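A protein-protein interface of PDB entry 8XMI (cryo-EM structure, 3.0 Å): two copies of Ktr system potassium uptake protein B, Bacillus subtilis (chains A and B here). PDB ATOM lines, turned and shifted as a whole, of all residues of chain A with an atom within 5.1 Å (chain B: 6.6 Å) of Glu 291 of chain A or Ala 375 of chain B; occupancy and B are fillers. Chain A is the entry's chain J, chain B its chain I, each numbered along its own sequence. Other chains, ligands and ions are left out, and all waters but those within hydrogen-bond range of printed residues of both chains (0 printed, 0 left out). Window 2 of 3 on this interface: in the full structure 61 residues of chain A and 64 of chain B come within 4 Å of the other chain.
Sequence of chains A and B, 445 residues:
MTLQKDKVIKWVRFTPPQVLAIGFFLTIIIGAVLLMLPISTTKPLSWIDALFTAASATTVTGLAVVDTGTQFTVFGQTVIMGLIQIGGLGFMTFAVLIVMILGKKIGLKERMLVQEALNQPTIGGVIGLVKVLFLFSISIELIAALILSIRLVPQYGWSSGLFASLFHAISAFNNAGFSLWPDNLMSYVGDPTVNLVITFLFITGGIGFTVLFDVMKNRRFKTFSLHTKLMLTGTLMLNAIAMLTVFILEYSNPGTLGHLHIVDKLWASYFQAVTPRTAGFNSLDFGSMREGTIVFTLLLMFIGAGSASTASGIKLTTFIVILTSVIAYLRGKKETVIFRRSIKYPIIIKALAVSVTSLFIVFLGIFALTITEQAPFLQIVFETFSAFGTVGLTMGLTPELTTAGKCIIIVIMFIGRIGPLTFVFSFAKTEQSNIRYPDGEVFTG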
ATOM      1  N   MET A 289      13.205 -27.956 -28.684  1.00  0.00           N
ATOM      2  CA  MET A 289      13.980 -27.039 -27.869  1.00  0.00           C
ATOM      3  C   MET A 289      15.471 -27.275 -28.078  1.00  0.00           C
ATOM      4  O   MET A 289      15.901 -28.321 -28.568  1.00  0.00           O
ATOM      5  CB  MET A 289      13.637 -27.199 -26.389  1.00  0.00           C
ATOM      6  CG  MET A 289      12.290 -26.635 -25.997  1.00  0.00           C
ATOM      7  SD  MET A 289      12.042 -26.640 -24.217  1.00  0.00           S
ATOM      8  CE  MET A 289      10.469 -25.797 -24.102  1.00  0.00           C
ATOM      9  N   ARG A 290      16.262 -26.279 -27.698  1.00  0.00           N
ATOM     10  CA  ARG A 290      17.705 -26.401 -27.803  1.00  0.00           C
ATOM     11  C   ARG A 290      18.239 -27.339 -26.728  1.00  0.00           C
ATOM     12  O   ARG A 290      17.569 -27.638 -25.738  1.00  0.00           O
ATOM     13  CB  ARG A 290      18.365 -25.029 -27.690  1.00  0.00           C
ATOM     14  CG  ARG A 290      17.954 -24.075 -28.788  1.00  0.00           C
ATOM     15  CD  ARG A 290      18.910 -22.909 -28.891  1.00  0.00           C
ATOM     16  NE  ARG A 290      18.704 -22.159 -30.123  1.00  0.00           N
ATOM     17  CZ  ARG A 290      17.954 -21.072 -30.219  1.00  0.00           C
ATOM     18  NH1 ARG A 290      17.332 -20.567 -29.166  1.00  0.00           N
ATOM     19  NH2 ARG A 290      17.828 -20.474 -31.399  1.00  0.00           N
ATOM     20  N   GLU A 291      19.468 -27.814 -26.938  1.00  0.00           N
ATOM     21  CA  GLU A 291      20.083 -28.709 -25.965  1.00  0.00           C
ATOM     22  C   GLU A 291      20.410 -27.992 -24.665  1.00  0.00           C
ATOM     23  O   GLU A 291      20.500 -28.636 -23.616  1.00  0.00           O
ATOM     24  CB  GLU A 291      21.349 -29.338 -26.543  1.00  0.00           C
ATOM     25  CG  GLU A 291      21.101 -30.342 -27.650  1.00  0.00           C
ATOM     26  CD  GLU A 291      22.373 -31.020 -28.113  1.00  0.00           C
ATOM     27  OE1 GLU A 291      23.467 -30.567 -27.717  1.00  0.00           O
ATOM     28  OE2 GLU A 291      22.277 -32.007 -28.871  1.00  0.00           O
ATOM     29  N   GLY A 292      20.601 -26.675 -24.710  1.00  0.00           N
ATOM     30  CA  GLY A 292      20.917 -25.944 -23.493  1.00  0.00           C
ATOM     31  C   GLY A 292      19.769 -25.923 -22.504  1.00  0.00           C
ATOM     32  O   GLY A 292      19.981 -26.022 -21.293  1.00  0.00           O
ATOM     33  N   THR A 293      18.540 -25.783 -23.003  1.00  0.00           N
ATOM     34  CA  THR A 293      17.379 -25.767 -22.121  1.00  0.00           C
ATOM     35  C   THR A 293      17.047 -27.161 -21.607  1.00  0.00           C
ATOM     36  O   THR A 293      16.533 -27.304 -20.492  1.00  0.00           O
ATOM     37  CB  THR A 293      16.178 -25.170 -22.850  1.00  0.00           C
ATOM     38  OG1 THR A 293      16.605 -24.052 -23.637  1.00  0.00           O
ATOM     39  CG2 THR A 293      15.139 -24.693 -21.858  1.00  0.00           C
ATOM     40  N   ILE A 294      17.326 -28.192 -22.403  1.00  0.00           N
ATOM     41  CA  ILE A 294      17.068 -29.564 -21.979  1.00  0.00           C
ATOM     42  C   ILE A 294      18.023 -29.971 -20.863  1.00  0.00           C
ATOM     43  O   ILE A 294      17.637 -30.682 -19.929  1.00  0.00           O
ATOM     44  CB  ILE A 294      17.161 -30.508 -23.190  1.00  0.00           C
ATOM     45  CG1 ILE A 294      16.102 -30.133 -24.223  1.00  0.00           C
ATOM     46  CG2 ILE A 294      16.984 -31.947 -22.773  1.00  0.00           C
ATOM     47  CD1 ILE A 294      16.232 -30.880 -25.520  1.00  0.00           C
ATOM     48  N   VAL A 295      19.280 -29.533 -20.942  1.00  0.00           N
ATOM     49  CA  VAL A 295      20.251 -29.845 -19.894  1.00  0.00           C
ATOM     50  C   VAL A 295      19.862 -29.177 -18.583  1.00  0.00           C
ATOM     51  O   VAL A 295      19.949 -29.785 -17.510  1.00  0.00           O
ATOM     52  CB  VAL A 295      21.668 -29.446 -20.344  1.00  0.00           C
ATOM     53  CG1 VAL A 295      22.640 -29.512 -19.184  1.00  0.00           C
ATOM     54  CG2 VAL A 295      22.130 -30.358 -21.451  1.00  0.00           C
ATOM     55  N   LEU A 378      20.408 -38.022 -26.094  1.00  0.00           N
ATOM     56  CA  LEU A 378      19.732 -36.967 -25.346  1.00  0.00           C
ATOM     57  C   LEU A 378      18.322 -37.386 -24.953  1.00  0.00           C
ATOM     58  O   LEU A 378      17.858 -37.065 -23.853  1.00  0.00           O
ATOM     59  CB  LEU A 378      19.700 -35.681 -26.166  1.00  0.00           C
ATOM     60  CG  LEU A 378      19.064 -34.459 -25.505  1.00  0.00           C
ATOM     61  CD1 LEU A 378      19.678 -34.190 -24.148  1.00  0.00           C
ATOM     62  CD2 LEU A 378      19.220 -33.254 -26.402  1.00  0.00           C
ATOM     63  N   PHE B 367      26.753 -27.852 -19.700  1.00  0.00           N
ATOM     64  CA  PHE B 367      25.790 -26.799 -20.002  1.00  0.00           C
ATOM     65  C   PHE B 367      26.394 -25.726 -20.896  1.00  0.00           C
ATOM     66  O   PHE B 367      25.764 -25.296 -21.867  1.00  0.00           O
ATOM     67  CB  PHE B 367      25.272 -26.185 -18.702  1.00  0.00           C
ATOM     68  CG  PHE B 367      24.245 -25.113 -18.902  1.00  0.00           C
ATOM     69  CD1 PHE B 367      22.929 -25.440 -19.167  1.00  0.00           C
ATOM     70  CD2 PHE B 367      24.591 -23.776 -18.811  1.00  0.00           C
ATOM     71  CE1 PHE B 367      21.983 -24.459 -19.348  1.00  0.00           C
ATOM     72  CE2 PHE B 367      23.648 -22.791 -18.993  1.00  0.00           C
ATOM     73  CZ  PHE B 367      22.343 -23.133 -19.260  1.00  0.00           C
ATOM     74  N   LEU B 369      28.959 -25.908 -22.929  1.00  0.00           N
ATOM     75  CA  LEU B 369      29.369 -26.378 -24.248  1.00  0.00           C
ATOM     76  C   LEU B 369      28.183 -26.561 -25.185  1.00  0.00           C
ATOM     77  O   LEU B 369      28.319 -26.356 -26.396  1.00  0.00           O
ATOM     78  CB  LEU B 369      30.152 -27.680 -24.120  1.00  0.00           C
ATOM     79  CG  LEU B 369      31.639 -27.545 -23.805  1.00  0.00           C
ATOM     80  CD1 LEU B 369      32.248 -28.910 -23.588  1.00  0.00           C
ATOM     81  CD2 LEU B 369      32.340 -26.828 -24.935  1.00  0.00           C
ATOM     82  N   THR B 370      27.024 -26.961 -24.657  1.00  0.00           N
ATOM     83  CA  THR B 370      25.837 -27.088 -25.496  1.00  0.00           C
ATOM     84  C   THR B 370      25.354 -25.732 -25.991  1.00  0.00           C
ATOM     85  O   THR B 370      24.806 -25.635 -27.094  1.00  0.00           O
ATOM     86  CB  THR B 370      24.721 -27.800 -24.733  1.00  0.00           C
ATOM     87  OG1 THR B 370      24.560 -27.195 -23.446  1.00  0.00           O
ATOM     88  CG2 THR B 370      25.049 -29.268 -24.558  1.00  0.00           C
ATOM     89  N   ILE B 371      25.535 -24.682 -25.187  1.00  0.00           N
ATOM     90  CA  ILE B 371      25.261 -23.327 -25.651  1.00  0.00           C
ATOM     91  C   ILE B 371      26.209 -22.952 -26.782  1.00  0.00           C
ATOM     92  O   ILE B 371      25.799 -22.365 -27.790  1.00  0.00           O
ATOM     93  CB  ILE B 371      25.366 -22.332 -24.481  1.00  0.00           C
ATOM     94  CG1 ILE B 371      24.461 -22.756 -23.326  1.00  0.00           C
ATOM     95  CG2 ILE B 371      25.015 -20.932 -24.939  1.00  0.00           C
ATOM     96  CD1 ILE B 371      23.011 -22.842 -23.695  1.00  0.00           C
ATOM     97  N   GLU B 373      28.848 -25.081 -28.573  1.00  0.00           N
ATOM     98  CA  GLU B 373      29.123 -25.999 -29.667  1.00  0.00           C
ATOM     99  C   GLU B 373      27.840 -26.546 -30.277  1.00  0.00           C
ATOM    100  O   GLU B 373      26.861 -26.809 -29.574  1.00  0.00           O
ATOM    101  CB  GLU B 373      29.992 -27.157 -29.180  1.00  0.00           C
ATOM    102  CG  GLU B 373      31.399 -26.742 -28.819  1.00  0.00           C
ATOM    103  CD  GLU B 373      32.109 -26.075 -29.975  1.00  0.00           C
ATOM    104  OE1 GLU B 373      32.107 -26.643 -31.087  1.00  0.00           O
ATOM    105  OE2 GLU B 373      32.661 -24.973 -29.776  1.00  0.00           O
ATOM    106  N   GLN B 374      27.855 -26.715 -31.595  1.00  0.00           N
ATOM    107  CA  GLN B 374      26.793 -27.407 -32.319  1.00  0.00           C
ATOM    108  C   GLN B 374      27.291 -28.822 -32.591  1.00  0.00           C
ATOM    109  O   GLN B 374      27.775 -29.124 -33.685  1.00  0.00           O
ATOM    110  CB  GLN B 374      26.436 -26.670 -33.605  1.00  0.00           C
ATOM    111  CG  GLN B 374      25.986 -25.236 -33.383  1.00  0.00           C
ATOM    112  CD  GLN B 374      24.785 -25.136 -32.461  1.00  0.00           C
ATOM    113  OE1 GLN B 374      23.844 -25.924 -32.558  1.00  0.00           O
ATOM    114  NE2 GLN B 374      24.815 -24.164 -31.555  1.00  0.00           N
ATOM    115  N   ALA B 375      27.171 -29.684 -31.590  1.00  0.00           N
ATOM    116  CA  ALA B 375      27.731 -31.026 -31.634  1.00  0.00           C
ATOM    117  C   ALA B 375      26.713 -31.989 -31.046  1.00  0.00           C
ATOM    118  O   ALA B 375      25.808 -31.568 -30.318  1.00  0.00           O
ATOM    119  CB  ALA B 375      29.054 -31.097 -30.861  1.00  0.00           C
ATOM    120  N   PRO B 376      26.812 -33.281 -31.366  1.00  0.00           N
ATOM    121  CA  PRO B 376      25.946 -34.265 -30.710  1.00  0.00           C
ATOM    122  C   PRO B 376      26.175 -34.292 -29.207  1.00  0.00           C
ATOM    123  O   PRO B 376      27.282 -34.061 -28.720  1.00  0.00           O
ATOM    124  CB  PRO B 376      26.356 -35.588 -31.362  1.00  0.00           C
ATOM    125  CG  PRO B 376      26.852 -35.190 -32.700  1.00  0.00           C
ATOM    126  CD  PRO B 376      27.542 -33.873 -32.500  1.00  0.00           C
ATOM    127  N   PHE B 377      25.095 -34.571 -28.474  1.00  0.00           N
ATOM    128  CA  PHE B 377      25.113 -34.446 -27.022  1.00  0.00           C
ATOM    129  C   PHE B 377      26.073 -35.427 -26.367  1.00  0.00           C
ATOM    130  O   PHE B 377      26.760 -35.064 -25.408  1.00  0.00           O
ATOM    131  CB  PHE B 377      23.705 -34.639 -26.471  1.00  0.00           C
ATOM    132  CG  PHE B 377      23.605 -34.473 -24.988  1.00  0.00           C
ATOM    133  CD1 PHE B 377      23.873 -33.254 -24.397  1.00  0.00           C
ATOM    134  CD2 PHE B 377      23.220 -35.531 -24.186  1.00  0.00           C
ATOM    135  CE1 PHE B 377      23.775 -33.099 -23.034  1.00  0.00           C
ATOM    136  CE2 PHE B 377      23.117 -35.379 -22.823  1.00  0.00           C
ATOM    137  CZ  PHE B 377      23.391 -34.160 -22.247  1.00  0.00           C
ATOM    138  N   LEU B 378      26.133 -36.665 -26.861  1.00  0.00           N
ATOM    139  CA  LEU B 378      27.007 -37.662 -26.249  1.00  0.00           C
ATOM    140  C   LEU B 378      28.474 -37.286 -26.410  1.00  0.00           C
ATOM    141  O   LEU B 378      29.291 -37.568 -25.528  1.00  0.00           O
ATOM    142  CB  LEU B 378      26.728 -39.040 -26.845  1.00  0.00           C
ATOM    143  CG  LEU B 378      27.495 -40.226 -26.257  1.00  0.00           C
ATOM    144  CD1 LEU B 378      27.443 -40.218 -24.742  1.00  0.00           C
ATOM    145  CD2 LEU B 378      26.948 -41.532 -26.795  1.00  0.00           C
ATOM    146  N   GLN B 379      28.828 -36.641 -27.524  1.00  0.00           N
ATOM    147  CA  GLN B 379      30.199 -36.175 -27.702  1.00  0.00           C
ATOM    148  C   GLN B 379      30.537 -35.039 -26.749  1.00  0.00           C
ATOM    149  O   GLN B 379      31.681 -34.932 -26.299  1.00  0.00           O
ATOM    150  CB  GLN B 379      30.420 -35.736 -29.147  1.00  0.00           C
ATOM    151  CG  GLN B 379      30.260 -36.856 -30.150  1.00  0.00           C
ATOM    152  CD  GLN B 379      30.653 -36.440 -31.547  1.00  0.00           C
ATOM    153  OE1 GLN B 379      31.050 -35.300 -31.779  1.00  0.00           O
ATOM    154  NE2 GLN B 379      30.547 -37.368 -32.489  1.00  0.00           N
ATOM    155  N   ILE B 380      29.567 -34.178 -26.443  1.00  0.00           N
ATOM    156  CA  ILE B 380      29.798 -33.089 -25.499  1.00  0.00           C
ATOM    157  C   ILE B 380      29.930 -33.625 -24.078  1.00  0.00           C
ATOM    158  O   ILE B 380      30.779 -33.169 -23.304  1.00  0.00           O
ATOM    159  CB  ILE B 380      28.674 -32.044 -25.626  1.00  0.00           C
ATOM    160  CG1 ILE B 380      28.788 -31.321 -26.967  1.00  0.00           C
ATOM    161  CG2 ILE B 380      28.712 -31.051 -24.484  1.00  0.00           C
ATOM    162  CD1 ILE B 380      27.690 -30.332 -27.218  1.00  0.00           C
ATOM    163  N   LEU B 397      35.414 -34.483 -31.110  1.00  0.00           N
ATOM    164  CA  LEU B 397      34.962 -33.122 -30.852  1.00  0.00           C
ATOM    165  C   LEU B 397      36.089 -32.112 -30.715  1.00  0.00           C
ATOM    166  O   LEU B 397      35.926 -30.971 -31.152  1.00  0.00           O
ATOM    167  CB  LEU B 397      34.104 -33.082 -29.579  1.00  0.00           C
ATOM    168  CG  LEU B 397      33.573 -31.715 -29.141  1.00  0.00           C
ATOM    169  CD1 LEU B 397      32.669 -31.137 -30.207  1.00  0.00           C
ATOM    170  CD2 LEU B 397      32.851 -31.794 -27.813  1.00  0.00           C
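Of the 13 printed residues of chain B, 5 touch a printed residue of chain A.
Of the 8 printed residues of chain A, 4 touch a printed residue of chain B.
Among the printed residues, no Asp or Glu carboxylate lies within 4 Å of a Lys or Arg side-chain nitrogen of the other chain.
Position printed for both chains: 378.
Of the 8 pairs that touch across the chains among the printed residues, none has its exchanged pair printed and touching as well.
Thr 370 of chain B touches Glu 291 of chain A (CG2 to OE1, 3.8 Å).
Ala 375 of chain B touches Glu 291 of chain A.
N of Phe 377 of chain B touches OE2 of Glu 291 of chain A, 3.8 Å away.
Gly 292 of chain A touches Phe 367 of chain B.
CA of Gly 292 of chain A touches OG1 of Thr 370 of chain B, at 3.9 Å.
Ile 371 of chain B touches Gly 292 of chain A.
Phe 377 of chain B touches Val 295 of chain A.
Phe 377 of chain B touches Leu 378 of chain A.
Glu 291 of chain A touches just these residues of chain B: Thr 370 (3.8 Å), Ala 375 (3.6 Å) and Phe 377 (3.8 Å).
Ala 375 of chain B touches just one residue of chain A: Glu 291.
Of the printed residues of chain A, Phe 367 of chain B touches Gly 292 (3.2 Å).
Of the printed residues of chain A, Thr 370 of chain B touches Glu 291 (3.8 Å) and Gly 292 (3.9 Å).
Gln 379 of chain B touches none of the printed residues of chain A.
Ile 380 of chain B touches none of the printed residues of chain A.
The backbone carbonyl oxygen (O) of Phe 367 of chain B sits at hydrogen-bond distance from the side-chain hydroxyl (OG1) of Thr 370 of chain B (2.7 Å).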
